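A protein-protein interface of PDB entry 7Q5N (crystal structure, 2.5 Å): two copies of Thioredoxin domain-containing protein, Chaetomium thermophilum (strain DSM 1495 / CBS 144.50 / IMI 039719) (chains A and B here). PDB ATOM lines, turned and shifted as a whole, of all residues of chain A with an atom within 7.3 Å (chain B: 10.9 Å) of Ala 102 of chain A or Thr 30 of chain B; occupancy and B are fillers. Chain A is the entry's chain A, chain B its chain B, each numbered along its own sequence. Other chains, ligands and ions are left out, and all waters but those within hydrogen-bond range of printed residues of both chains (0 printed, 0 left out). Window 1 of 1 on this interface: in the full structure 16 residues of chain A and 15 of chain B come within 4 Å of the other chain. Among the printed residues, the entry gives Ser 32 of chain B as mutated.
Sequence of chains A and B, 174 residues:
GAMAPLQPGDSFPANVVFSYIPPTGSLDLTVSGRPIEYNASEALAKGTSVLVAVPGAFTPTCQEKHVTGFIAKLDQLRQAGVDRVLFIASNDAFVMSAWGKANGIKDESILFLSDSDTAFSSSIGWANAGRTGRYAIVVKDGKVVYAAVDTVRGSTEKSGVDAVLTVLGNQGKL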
ATOM      1  N   LEU A  27     -23.778   6.128   2.240  1.00  0.00           N
ATOM      2  CA  LEU A  27     -23.645   5.327   3.448  1.00  0.00           C
ATOM      3  C   LEU A  27     -22.323   5.597   4.161  1.00  0.00           C
ATOM      4  O   LEU A  27     -21.905   4.808   5.014  1.00  0.00           O
ATOM      5  CB  LEU A  27     -23.776   3.843   3.115  1.00  0.00           C
ATOM      6  CG  LEU A  27     -25.193   3.266   3.026  1.00  0.00           C
ATOM      7  CD1 LEU A  27     -26.159   4.265   2.449  1.00  0.00           C
ATOM      8  CD2 LEU A  27     -25.219   1.989   2.194  1.00  0.00           C
ATOM      9  N   LEU A  29     -20.233   7.218   6.877  1.00  0.00           N
ATOM     10  CA  LEU A  29     -20.462   7.812   8.186  1.00  0.00           C
ATOM     11  C   LEU A  29     -19.457   8.901   8.532  1.00  0.00           C
ATOM     12  O   LEU A  29     -19.668   9.626   9.510  1.00  0.00           O
ATOM     13  CB  LEU A  29     -20.423   6.722   9.264  1.00  0.00           C
ATOM     14  CG  LEU A  29     -21.709   5.906   9.427  1.00  0.00           C
ATOM     15  CD1 LEU A  29     -21.781   4.803   8.383  1.00  0.00           C
ATOM     16  CD2 LEU A  29     -21.799   5.328  10.831  1.00  0.00           C
ATOM     17  N   PHE A  58     -27.562   3.742  18.591  1.00  0.00           N
ATOM     18  CA  PHE A  58     -26.412   2.856  18.722  1.00  0.00           C
ATOM     19  C   PHE A  58     -26.414   2.057  20.020  1.00  0.00           C
ATOM     20  O   PHE A  58     -25.370   1.532  20.424  1.00  0.00           O
ATOM     21  CB  PHE A  58     -25.097   3.637  18.609  1.00  0.00           C
ATOM     22  CG  PHE A  58     -24.817   4.159  17.236  1.00  0.00           C
ATOM     23  CD1 PHE A  58     -24.354   3.319  16.242  1.00  0.00           C
ATOM     24  CD2 PHE A  58     -25.007   5.501  16.938  1.00  0.00           C
ATOM     25  CE1 PHE A  58     -24.091   3.804  14.973  1.00  0.00           C
ATOM     26  CE2 PHE A  58     -24.747   5.986  15.676  1.00  0.00           C
ATOM     27  CZ  PHE A  58     -24.286   5.139  14.693  1.00  0.00           C
ATOM     28  N   THR A  59     -27.553   1.946  20.691  1.00  0.00           N
ATOM     29  CA  THR A  59     -27.629   1.108  21.880  1.00  0.00           C
ATOM     30  C   THR A  59     -28.228  -0.252  21.536  1.00  0.00           C
ATOM     31  O   THR A  59     -28.875  -0.416  20.493  1.00  0.00           O
ATOM     32  CB  THR A  59     -28.462   1.787  22.969  1.00  0.00           C
ATOM     33  OG1 THR A  59     -29.839   1.802  22.582  1.00  0.00           O
ATOM     34  CG2 THR A  59     -27.986   3.211  23.199  1.00  0.00           C
ATOM     35  N   PRO A  60     -28.049  -1.255  22.408  1.00  0.00           N
ATOM     36  CA  PRO A  60     -28.363  -2.642  22.016  1.00  0.00           C
ATOM     37  C   PRO A  60     -29.811  -2.889  21.616  1.00  0.00           C
ATOM     38  O   PRO A  60     -30.070  -3.321  20.487  1.00  0.00           O
ATOM     39  CB  PRO A  60     -27.990  -3.455  23.267  1.00  0.00           C
ATOM     40  CG  PRO A  60     -27.024  -2.602  24.022  1.00  0.00           C
ATOM     41  CD  PRO A  60     -27.463  -1.177  23.757  1.00  0.00           C
ATOM     42  N   GLN A  63     -31.126  -0.833  18.782  1.00  0.00           N
ATOM     43  CA  GLN A  63     -30.534  -1.249  17.519  1.00  0.00           C
ATOM     44  C   GLN A  63     -30.949  -2.657  17.112  1.00  0.00           C
ATOM     45  O   GLN A  63     -31.584  -2.846  16.075  1.00  0.00           O
ATOM     46  CB  GLN A  63     -29.009  -1.177  17.614  1.00  0.00           C
ATOM     47  CG  GLN A  63     -28.270  -1.768  16.422  1.00  0.00           C
ATOM     48  CD  GLN A  63     -28.755  -1.212  15.096  1.00  0.00           C
ATOM     49  OE1 GLN A  63     -29.359  -0.140  15.039  1.00  0.00           O
ATOM     50  NE2 GLN A  63     -28.495  -1.944  14.018  1.00  0.00           N
ATOM     51  N   GLU A  64     -30.594  -3.642  17.938  1.00  0.00           N
ATOM     52  CA  GLU A  64     -30.692  -5.042  17.539  1.00  0.00           C
ATOM     53  C   GLU A  64     -32.124  -5.556  17.457  1.00  0.00           C
ATOM     54  O   GLU A  64     -32.337  -6.627  16.880  1.00  0.00           O
ATOM     55  CB  GLU A  64     -29.886  -5.910  18.512  1.00  0.00           C
ATOM     56  CG  GLU A  64     -28.383  -5.628  18.481  1.00  0.00           C
ATOM     57  CD  GLU A  64     -27.686  -5.981  19.784  1.00  0.00           C
ATOM     58  OE1 GLU A  64     -28.258  -6.759  20.581  1.00  0.00           O
ATOM     59  OE2 GLU A  64     -26.560  -5.484  20.011  1.00  0.00           O
ATOM     60  N   THR A  68     -34.277  -2.626  13.608  1.00  0.00           N
ATOM     61  CA  THR A  68     -34.111  -3.751  12.693  1.00  0.00           C
ATOM     62  C   THR A  68     -35.455  -4.358  12.305  1.00  0.00           C
ATOM     63  O   THR A  68     -35.628  -4.812  11.168  1.00  0.00           O
ATOM     64  CB  THR A  68     -33.217  -4.820  13.315  1.00  0.00           C
ATOM     65  OG1 THR A  68     -33.697  -5.138  14.627  1.00  0.00           O
ATOM     66  CG2 THR A  68     -31.781  -4.332  13.408  1.00  0.00           C
ATOM     67  N   ILE A  71     -37.044  -2.009   9.649  1.00  0.00           N
ATOM     68  CA  ILE A  71     -36.326  -2.127   8.381  1.00  0.00           C
ATOM     69  C   ILE A  71     -36.671  -3.446   7.700  1.00  0.00           C
ATOM     70  O   ILE A  71     -36.838  -3.504   6.476  1.00  0.00           O
ATOM     71  CB  ILE A  71     -34.807  -1.989   8.614  1.00  0.00           C
ATOM     72  CG1 ILE A  71     -34.457  -0.560   9.020  1.00  0.00           C
ATOM     73  CG2 ILE A  71     -34.024  -2.379   7.371  1.00  0.00           C
ATOM     74  CD1 ILE A  71     -33.114  -0.440   9.704  1.00  0.00           C
ATOM     75  N   MET A  96     -27.948  10.789  14.633  1.00  0.00           N
ATOM     76  CA  MET A  96     -29.076  10.094  14.021  1.00  0.00           C
ATOM     77  C   MET A  96     -28.776   9.739  12.572  1.00  0.00           C
ATOM     78  O   MET A  96     -29.047   8.613  12.131  1.00  0.00           O
ATOM     79  CB  MET A  96     -30.332  10.960  14.114  1.00  0.00           C
ATOM     80  CG  MET A  96     -30.837  11.151  15.539  1.00  0.00           C
ATOM     81  SD  MET A  96     -31.167   9.564  16.388  1.00  0.00           S
ATOM     82  CE  MET A  96     -32.625   9.016  15.501  1.00  0.00           C
ATOM     83  N   SER A  97     -28.205  10.685  11.816  1.00  0.00           N
ATOM     84  CA  SER A  97     -27.849  10.408  10.430  1.00  0.00           C
ATOM     85  C   SER A  97     -26.852   9.263  10.337  1.00  0.00           C
ATOM     86  O   SER A  97     -26.969   8.396   9.465  1.00  0.00           O
ATOM     87  CB  SER A  97     -27.278  11.675   9.780  1.00  0.00           C
ATOM     88  OG  SER A  97     -26.915  11.447   8.428  1.00  0.00           O
ATOM     89  N   ALA A  98     -25.864   9.241  11.231  1.00  0.00           N
ATOM     90  CA  ALA A  98     -24.905   8.140  11.240  1.00  0.00           C
ATOM     91  C   ALA A  98     -25.563   6.819  11.630  1.00  0.00           C
ATOM     92  O   ALA A  98     -25.167   5.760  11.128  1.00  0.00           O
ATOM     93  CB  ALA A  98     -23.752   8.452  12.195  1.00  0.00           C
ATOM     94  N   TRP A  99     -26.557   6.859  12.519  1.00  0.00           N
ATOM     95  CA  TRP A  99     -27.257   5.633  12.897  1.00  0.00           C
ATOM     96  C   TRP A  99     -28.038   5.067  11.717  1.00  0.00           C
ATOM     97  O   TRP A  99     -27.972   3.867  11.430  1.00  0.00           O
ATOM     98  CB  TRP A  99     -28.181   5.912  14.083  1.00  0.00           C
ATOM     99  CG  TRP A  99     -28.703   4.682  14.777  1.00  0.00           C
ATOM    100  CD1 TRP A  99     -28.021   3.525  15.025  1.00  0.00           C
ATOM    101  CD2 TRP A  99     -30.018   4.496  15.314  1.00  0.00           C
ATOM    102  NE1 TRP A  99     -28.832   2.635  15.676  1.00  0.00           N
ATOM    103  CE2 TRP A  99     -30.063   3.206  15.864  1.00  0.00           C
ATOM    104  CE3 TRP A  99     -31.161   5.297  15.376  1.00  0.00           C
ATOM    105  CZ2 TRP A  99     -31.208   2.692  16.479  1.00  0.00           C
ATOM    106  CZ3 TRP A  99     -32.294   4.792  15.977  1.00  0.00           C
ATOM    107  CH2 TRP A  99     -32.313   3.500  16.522  1.00  0.00           C
ATOM    108  N   GLY A 100     -28.775   5.923  11.008  1.00  0.00           N
ATOM    109  CA  GLY A 100     -29.502   5.458   9.836  1.00  0.00           C
ATOM    110  C   GLY A 100     -28.587   4.852   8.788  1.00  0.00           C
ATOM    111  O   GLY A 100     -28.873   3.789   8.232  1.00  0.00           O
ATOM    112  N   LYS A 101     -27.472   5.527   8.500  1.00  0.00           N
ATOM    113  CA  LYS A 101     -26.503   4.976   7.558  1.00  0.00           C
ATOM    114  C   LYS A 101     -26.000   3.617   8.032  1.00  0.00           C
ATOM    115  O   LYS A 101     -25.927   2.660   7.256  1.00  0.00           O
ATOM    116  CB  LYS A 101     -25.331   5.940   7.377  1.00  0.00           C
ATOM    117  CG  LYS A 101     -25.675   7.232   6.666  1.00  0.00           C
ATOM    118  CD  LYS A 101     -24.528   8.216   6.803  1.00  0.00           C
ATOM    119  CE  LYS A 101     -24.809   9.518   6.094  1.00  0.00           C
ATOM    120  NZ  LYS A 101     -23.603  10.400   6.088  1.00  0.00           N
ATOM    121  N   ALA A 102     -25.635   3.523   9.310  1.00  0.00           N
ATOM    122  CA  ALA A 102     -25.169   2.255   9.858  1.00  0.00           C
ATOM    123  C   ALA A 102     -26.167   1.128   9.631  1.00  0.00           C
ATOM    124  O   ALA A 102     -25.782  -0.043   9.683  1.00  0.00           O
ATOM    125  CB  ALA A 102     -24.884   2.400  11.355  1.00  0.00           C
ATOM    126  N   ASN A 103     -27.433   1.460   9.378  1.00  0.00           N
ATOM    127  CA  ASN A 103     -28.471   0.482   9.087  1.00  0.00           C
ATOM    128  C   ASN A 103     -28.797   0.404   7.599  1.00  0.00           C
ATOM    129  O   ASN A 103     -29.843  -0.142   7.225  1.00  0.00           O
ATOM    130  CB  ASN A 103     -29.733   0.805   9.887  1.00  0.00           C
ATOM    131  CG  ASN A 103     -29.644   0.330  11.330  1.00  0.00           C
ATOM    132  OD1 ASN A 103     -29.733  -0.866  11.606  1.00  0.00           O
ATOM    133  ND2 ASN A 103     -29.461   1.268  12.256  1.00  0.00           N
ATOM    134  N   GLY A 104     -27.930   0.950   6.744  1.00  0.00           N
ATOM    135  CA  GLY A 104     -28.100   0.831   5.311  1.00  0.00           C
ATOM    136  C   GLY A 104     -29.205   1.662   4.708  1.00  0.00           C
ATOM    137  O   GLY A 104     -29.519   1.483   3.526  1.00  0.00           O
ATOM    138  N   ILE A 105     -29.809   2.567   5.471  1.00  0.00           N
ATOM    139  CA  ILE A 105     -30.889   3.404   4.955  1.00  0.00           C
ATOM    140  C   ILE A 105     -30.264   4.596   4.227  1.00  0.00           C
ATOM    141  O   ILE A 105     -29.668   5.478   4.851  1.00  0.00           O
ATOM    142  CB  ILE A 105     -31.827   3.864   6.076  1.00  0.00           C
ATOM    143  CG1 ILE A 105     -32.510   2.657   6.732  1.00  0.00           C
ATOM    144  CG2 ILE A 105     -32.871   4.843   5.538  1.00  0.00           C
ATOM    145  CD1 ILE A 105     -33.359   1.821   5.787  1.00  0.00           C
ATOM    146  N   ILE B  21     -16.513   1.669  25.872  1.00  0.00           N
ATOM    147  CA  ILE B  21     -16.619   0.275  25.451  1.00  0.00           C
ATOM    148  C   ILE B  21     -15.246  -0.153  24.947  1.00  0.00           C
ATOM    149  O   ILE B  21     -14.816   0.320  23.882  1.00  0.00           O
ATOM    150  CB  ILE B  21     -17.693   0.099  24.366  1.00  0.00           C
ATOM    151  CG1 ILE B  21     -19.066   0.480  24.938  1.00  0.00           C
ATOM    152  CG2 ILE B  21     -17.678  -1.317  23.813  1.00  0.00           C
ATOM    153  CD1 ILE B  21     -20.245  -0.012  24.137  1.00  0.00           C
ATOM    154  N   THR B  24     -12.987  -4.298  20.656  1.00  0.00           N
ATOM    155  CA  THR B  24     -12.960  -5.745  20.503  1.00  0.00           C
ATOM    156  C   THR B  24     -12.265  -6.201  19.227  1.00  0.00           C
ATOM    157  O   THR B  24     -12.024  -7.402  19.070  1.00  0.00           O
ATOM    158  CB  THR B  24     -14.391  -6.303  20.511  1.00  0.00           C
ATOM    159  OG1 THR B  24     -15.124  -5.770  19.399  1.00  0.00           O
ATOM    160  CG2 THR B  24     -15.104  -5.939  21.808  1.00  0.00           C
ATOM    161  N   SER B  26     -13.690  -5.238  16.232  1.00  0.00           N
ATOM    162  CA  SER B  26     -14.761  -5.169  15.252  1.00  0.00           C
ATOM    163  C   SER B  26     -14.943  -3.744  14.737  1.00  0.00           C
ATOM    164  O   SER B  26     -14.717  -2.767  15.454  1.00  0.00           O
ATOM    165  CB  SER B  26     -16.074  -5.664  15.859  1.00  0.00           C
ATOM    166  OG  SER B  26     -17.168  -5.395  15.000  1.00  0.00           O
ATOM    167  N   LEU B  27     -15.352  -3.641  13.471  1.00  0.00           N
ATOM    168  CA  LEU B  27     -15.784  -2.388  12.876  1.00  0.00           C
ATOM    169  C   LEU B  27     -17.285  -2.380  12.612  1.00  0.00           C
ATOM    170  O   LEU B  27     -17.780  -1.537  11.855  1.00  0.00           O
ATOM    171  CB  LEU B  27     -15.017  -2.119  11.583  1.00  0.00           C
ATOM    172  CG  LEU B  27     -13.692  -1.363  11.729  1.00  0.00           C
ATOM    173  CD1 LEU B  27     -12.913  -1.888  12.915  1.00  0.00           C
ATOM    174  CD2 LEU B  27     -12.859  -1.483  10.472  1.00  0.00           C
ATOM    175  N   ASP B  28     -18.019  -3.303  13.226  1.00  0.00           N
ATOM    176  CA  ASP B  28     -19.459  -3.413  13.024  1.00  0.00           C
ATOM    177  C   ASP B  28     -20.169  -2.405  13.918  1.00  0.00           C
ATOM    178  O   ASP B  28     -20.114  -2.508  15.149  1.00  0.00           O
ATOM    179  CB  ASP B  28     -19.927  -4.835  13.324  1.00  0.00           C
ATOM    180  CG  ASP B  28     -21.284  -5.148  12.717  1.00  0.00           C
ATOM    181  OD1 ASP B  28     -21.670  -4.490  11.726  1.00  0.00           O
ATOM    182  OD2 ASP B  28     -21.961  -6.062  13.229  1.00  0.00           O
ATOM    183  N   LEU B  29     -20.834  -1.430  13.297  1.00  0.00           N
ATOM    184  CA  LEU B  29     -21.480  -0.364  14.049  1.00  0.00           C
ATOM    185  C   LEU B  29     -22.773  -0.817  14.707  1.00  0.00           C
ATOM    186  O   LEU B  29     -23.245  -0.154  15.637  1.00  0.00           O
ATOM    187  CB  LEU B  29     -21.771   0.825  13.129  1.00  0.00           C
ATOM    188  CG  LEU B  29     -20.634   1.466  12.328  1.00  0.00           C
ATOM    189  CD1 LEU B  29     -19.375   1.596  13.168  1.00  0.00           C
ATOM    190  CD2 LEU B  29     -20.340   0.707  11.036  1.00  0.00           C
ATOM    191  N   THR B  30     -23.349  -1.927  14.248  1.00  0.00           N
ATOM    192  CA  THR B  30     -24.630  -2.407  14.745  1.00  0.00           C
ATOM    193  C   THR B  30     -24.504  -3.304  15.971  1.00  0.00           C
ATOM    194  O   THR B  30     -25.530  -3.661  16.561  1.00  0.00           O
ATOM    195  CB  THR B  30     -25.365  -3.174  13.639  1.00  0.00           C
ATOM    196  OG1 THR B  30     -24.569  -4.294  13.220  1.00  0.00           O
ATOM    197  CG2 THR B  30     -25.633  -2.266  12.443  1.00  0.00           C
ATOM    198  N   VAL B  31     -23.290  -3.672  16.372  1.00  0.00           N
ATOM    199  CA  VAL B  31     -23.074  -4.558  17.511  1.00  0.00           C
ATOM    200  C   VAL B  31     -22.405  -3.748  18.611  1.00  0.00           C
ATOM    201  O   VAL B  31     -21.241  -3.349  18.480  1.00  0.00           O
ATOM    202  CB  VAL B  31     -22.229  -5.782  17.140  1.00  0.00           C
ATOM    203  CG1 VAL B  31     -22.073  -6.705  18.346  1.00  0.00           C
ATOM    204  CG2 VAL B  31     -22.863  -6.526  15.994  1.00  0.00           C
ATOM    205  N   SER B  32     -23.133  -3.520  19.698  1.00  0.00           N
ATOM    206  CA  SER B  32     -22.614  -2.785  20.839  1.00  0.00           C
ATOM    207  C   SER B  32     -22.006  -3.743  21.855  1.00  0.00           C
ATOM    208  O   SER B  32     -22.544  -4.825  22.108  1.00  0.00           O
ATOM    209  CB  SER B  32     -23.731  -1.975  21.499  1.00  0.00           C
ATOM    210  OG  SER B  32     -24.555  -1.348  20.526  1.00  0.00           O
ATOM    211  N   GLY B  33     -20.875  -3.341  22.429  1.00  0.00           N
ATOM    212  CA  GLY B  33     -20.292  -4.032  23.561  1.00  0.00           C
ATOM    213  C   GLY B  33     -20.975  -3.619  24.845  1.00  0.00           C
ATOM    214  O   GLY B  33     -22.151  -3.228  24.853  1.00  0.00           O
ATOM    215  N   ARG B  34     -20.230  -3.685  25.947  1.00  0.00           N
ATOM    216  CA  ARG B  34     -20.753  -3.301  27.254  1.00  0.00           C
ATOM    217  C   ARG B  34     -19.888  -2.206  27.862  1.00  0.00           C
ATOM    218  O   ARG B  34     -18.686  -2.429  28.084  1.00  0.00           O
ATOM    219  CB  ARG B  34     -20.814  -4.511  28.193  1.00  0.00           C
ATOM    220  CG  ARG B  34     -21.767  -4.306  29.359  1.00  0.00           C
ATOM    221  CD  ARG B  34     -21.251  -4.927  30.648  1.00  0.00           C
ATOM    222  NE  ARG B  34     -21.966  -4.401  31.807  1.00  0.00           N
ATOM    223  CZ  ARG B  34     -21.388  -3.909  32.897  1.00  0.00           C
ATOM    224  NH1 ARG B  34     -20.072  -3.885  33.035  1.00  0.00           N
ATOM    225  NH2 ARG B  34     -22.153  -3.430  33.874  1.00  0.00           N
ATOM    226  N   PHE B  58     -19.482  12.502  15.462  1.00  0.00           N
ATOM    227  CA  PHE B  58     -20.129  12.503  14.154  1.00  0.00           C
ATOM    228  C   PHE B  58     -20.451  13.904  13.629  1.00  0.00           C
ATOM    229  O   PHE B  58     -21.191  14.031  12.644  1.00  0.00           O
ATOM    230  CB  PHE B  58     -21.411  11.663  14.170  1.00  0.00           C
ATOM    231  CG  PHE B  58     -21.165  10.193  14.259  1.00  0.00           C
ATOM    232  CD1 PHE B  58     -20.720   9.485  13.159  1.00  0.00           C
ATOM    233  CD2 PHE B  58     -21.379   9.512  15.454  1.00  0.00           C
ATOM    234  CE1 PHE B  58     -20.489   8.121  13.242  1.00  0.00           C
ATOM    235  CE2 PHE B  58     -21.147   8.156  15.543  1.00  0.00           C
ATOM    236  CZ  PHE B  58     -20.705   7.456  14.437  1.00  0.00           C
ATOM    237  N   PHE B  94     -21.782   4.267  23.898  1.00  0.00           N
ATOM    238  CA  PHE B  94     -22.169   3.550  22.687  1.00  0.00           C
ATOM    239  C   PHE B  94     -21.881   4.387  21.449  1.00  0.00           C
ATOM    240  O   PHE B  94     -21.307   3.897  20.469  1.00  0.00           O
ATOM    241  CB  PHE B  94     -23.653   3.172  22.749  1.00  0.00           C
ATOM    242  CG  PHE B  94     -23.999   2.248  23.879  1.00  0.00           C
ATOM    243  CD1 PHE B  94     -23.751   0.887  23.778  1.00  0.00           C
ATOM    244  CD2 PHE B  94     -24.569   2.735  25.042  1.00  0.00           C
ATOM    245  CE1 PHE B  94     -24.070   0.025  24.818  1.00  0.00           C
ATOM    246  CE2 PHE B  94     -24.889   1.874  26.091  1.00  0.00           C
ATOM    247  CZ  PHE B  94     -24.639   0.523  25.975  1.00  0.00           C
ATOM    248  N   VAL B  95     -22.266   5.665  21.480  1.00  0.00           N
ATOM    249  CA  VAL B  95     -22.032   6.539  20.334  1.00  0.00           C
ATOM    250  C   VAL B  95     -20.537   6.722  20.095  1.00  0.00           C
ATOM    251  O   VAL B  95     -20.063   6.659  18.957  1.00  0.00           O
ATOM    252  CB  VAL B  95     -22.741   7.891  20.549  1.00  0.00           C
ATOM    253  CG1 VAL B  95     -22.382   8.864  19.444  1.00  0.00           C
ATOM    254  CG2 VAL B  95     -24.253   7.691  20.628  1.00  0.00           C
ATOM    255  N   SER B  97     -18.134   4.683  20.776  1.00  0.00           N
ATOM    256  CA  SER B  97     -17.572   3.466  20.201  1.00  0.00           C
ATOM    257  C   SER B  97     -17.904   3.361  18.720  1.00  0.00           C
ATOM    258  O   SER B  97     -17.060   2.951  17.914  1.00  0.00           O
ATOM    259  CB  SER B  97     -18.088   2.237  20.956  1.00  0.00           C
ATOM    260  OG  SER B  97     -17.590   1.034  20.385  1.00  0.00           O
ATOM    261  N   ALA B  98     -19.130   3.725  18.339  1.00  0.00           N
ATOM    262  CA  ALA B  98     -19.490   3.709  16.923  1.00  0.00           C
ATOM    263  C   ALA B  98     -18.689   4.746  16.139  1.00  0.00           C
ATOM    264  O   ALA B  98     -18.319   4.510  14.981  1.00  0.00           O
ATOM    265  CB  ALA B  98     -20.988   3.959  16.758  1.00  0.00           C
ATOM    266  N   TRP B  99     -18.420   5.903  16.750  1.00  0.00           N
ATOM    267  CA  TRP B  99     -17.592   6.910  16.093  1.00  0.00           C
ATOM    268  C   TRP B  99     -16.191   6.367  15.834  1.00  0.00           C
ATOM    269  O   TRP B  99     -15.651   6.507  14.732  1.00  0.00           O
ATOM    270  CB  TRP B  99     -17.536   8.177  16.950  1.00  0.00           C
ATOM    271  CG  TRP B  99     -17.009   9.386  16.235  1.00  0.00           C
ATOM    272  CD1 TRP B  99     -17.240   9.737  14.937  1.00  0.00           C
ATOM    273  CD2 TRP B  99     -16.166  10.410  16.785  1.00  0.00           C
ATOM    274  NE1 TRP B  99     -16.589  10.909  14.646  1.00  0.00           N
ATOM    275  CE2 TRP B  99     -15.925  11.344  15.761  1.00  0.00           C
ATOM    276  CE3 TRP B  99     -15.591  10.621  18.042  1.00  0.00           C
ATOM    277  CZ2 TRP B  99     -15.128  12.481  15.953  1.00  0.00           C
ATOM    278  CZ3 TRP B  99     -14.810  11.733  18.238  1.00  0.00           C
ATOM    279  CH2 TRP B  99     -14.582  12.661  17.194  1.00  0.00           C
ATOM    280  N   LYS B 101     -15.286   3.213  15.526  1.00  0.00           N
ATOM    281  CA  LYS B 101     -15.385   2.229  14.454  1.00  0.00           C
ATOM    282  C   LYS B 101     -15.542   2.907  13.097  1.00  0.00           C
ATOM    283  O   LYS B 101     -14.891   2.520  12.119  1.00  0.00           O
ATOM    284  CB  LYS B 101     -16.559   1.285  14.709  1.00  0.00           C
ATOM    285  CG  LYS B 101     -16.400   0.362  15.912  1.00  0.00           C
ATOM    286  CD  LYS B 101     -17.740  -0.272  16.266  1.00  0.00           C
ATOM    287  CE  LYS B 101     -17.649  -1.177  17.474  1.00  0.00           C
ATOM    288  NZ  LYS B 101     -18.935  -1.893  17.706  1.00  0.00           N
ATOM    289  N   ALA B 102     -16.409   3.919  13.017  1.00  0.00           N
ATOM    290  CA  ALA B 102     -16.608   4.622  11.753  1.00  0.00           C
ATOM    291  C   ALA B 102     -15.299   5.160  11.199  1.00  0.00           C
ATOM    292  O   ALA B 102     -15.171   5.345   9.984  1.00  0.00           O
ATOM    293  CB  ALA B 102     -17.605   5.766  11.935  1.00  0.00           C
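The backbone carbonyl oxygen (O) of Phe 58 of chain A lies within hydrogen-bond range of the side-chain hydroxyl (OG) of Ser 32 of chain B, at 3.0 Å.
OD1 of Asn 103 of chain A is in hydrogen-bond range of NE2 of Gln 63 of chain A, 2.9 Å away.
OG1 of Thr 68 of chain A lies within hydrogen-bond range of O of Glu 64 of chain A, 3.0 Å away.
The indole nitrogen of Trp 99 of chain A lies within hydrogen-bond range of the side-chain amide oxygen of Gln 63 of chain A, at 2.9 Å.
The side-chain hydroxyl (OG1) of Thr 30 of chain B sits close to the side-chain carboxylate (OD2) of Asp 28 of chain B.
O of Gln 63 of chain A lies close to OG1 of Thr 68 of chain A (3.4 Å).
O of Phe 58 of chain A touches CB of Phe 94 of chain B, 3.3 Å away.
CB of Ala 98 of chain B touches CD1 of Phe 58 of chain A, at 3.5 Å.
Thr 59 of chain A touches Ser 32 of chain B (C to OG, 3.96 Å).
CG2 of Thr 59 of chain A touches CD2 of Phe 94 of chain B (3.9 Å).
Ser 32 of chain B touches Pro 60 of chain A.
Gln 63 of chain A touches Thr 30 of chain B.
Thr 30 of chain B touches Glu 64 of chain A.
Glu 64 of chain A touches Ser 32 of chain B (OE2 to N, 3.96 Å).
CD1 of Phe 58 of chain B touches CB of Ala 98 of chain A, at 3.3 Å.
CG2 of Thr 30 of chain B touches O of Ala 102 of chain A, 3.5 Å away.
Gln 63 of chain A touches just one residue of chain B: Thr 30.
Of chain B, only Phe 58 (3.3 Å) comes within 4 Å of Ala 98 of chain A.
No residue of chain B comes within 4 Å of Gly 100 of chain A.
Ala 102 of chain A touches just these residues of chain B: Leu 29 (3.9 Å) and Thr 30 (3.5 Å).
Thr 30 of chain B touches three residues of chain A.
Printed residues of chain A within 4 Å of Ser 32 of chain B: Phe 58 (3.0 Å), Thr 59 (3.96 Å), Pro 60 (3.97 Å) and Glu 64 (3.96 Å).
Of the printed residues of chain A, Phe 94 of chain B touches Phe 58, Thr 59 and Pro 60.
The nearest residue of chain B that does not touch Ala 102 of chain A is Asp 28 of chain B (6.4 Å).
The nearest residue of chain A that does not touch Thr 30 of chain B is Asn 103 of chain A (4.4 Å).
The nearest printed residue of chain B that does not touch Glu 64 of chain A is Val 31 of chain B (4.4 Å).
Printed residues of chain A that touch a printed residue of chain B: Leu 29, Phe 58, Thr 59, Pro 60, Gln 63, Glu 64, Ala 98 and Ala 102.
Hydrophobic or aromatic side chains of chain A that line the printed part of chain B: Leu 29, Phe 58, Pro 60, Ala 98 and Ala 102.
Along chain A the printed residues that touch a printed residue of chain B span positions 29 to 102.
Among the printed residues, 16 pairs touch across the chains.
Leu 29 of chain A touches Phe 58 of chain B, and with the chains exchanged Phe 58 of chain A touches Leu 29 of chain B.
Leu 29 of chain A touches Ala 102 of chain B, and with the chains exchanged Ala 102 of chain A touches Leu 29 of chain B.
Phe 58 of chain A touches Ala 98 of chain B, and with the chains exchanged Ala 98 of chain A touches Phe 58 of chain B.
Of the 16 pairs that touch across the chains among the printed residues, 6 have their exchanged pair printed and touching as well.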
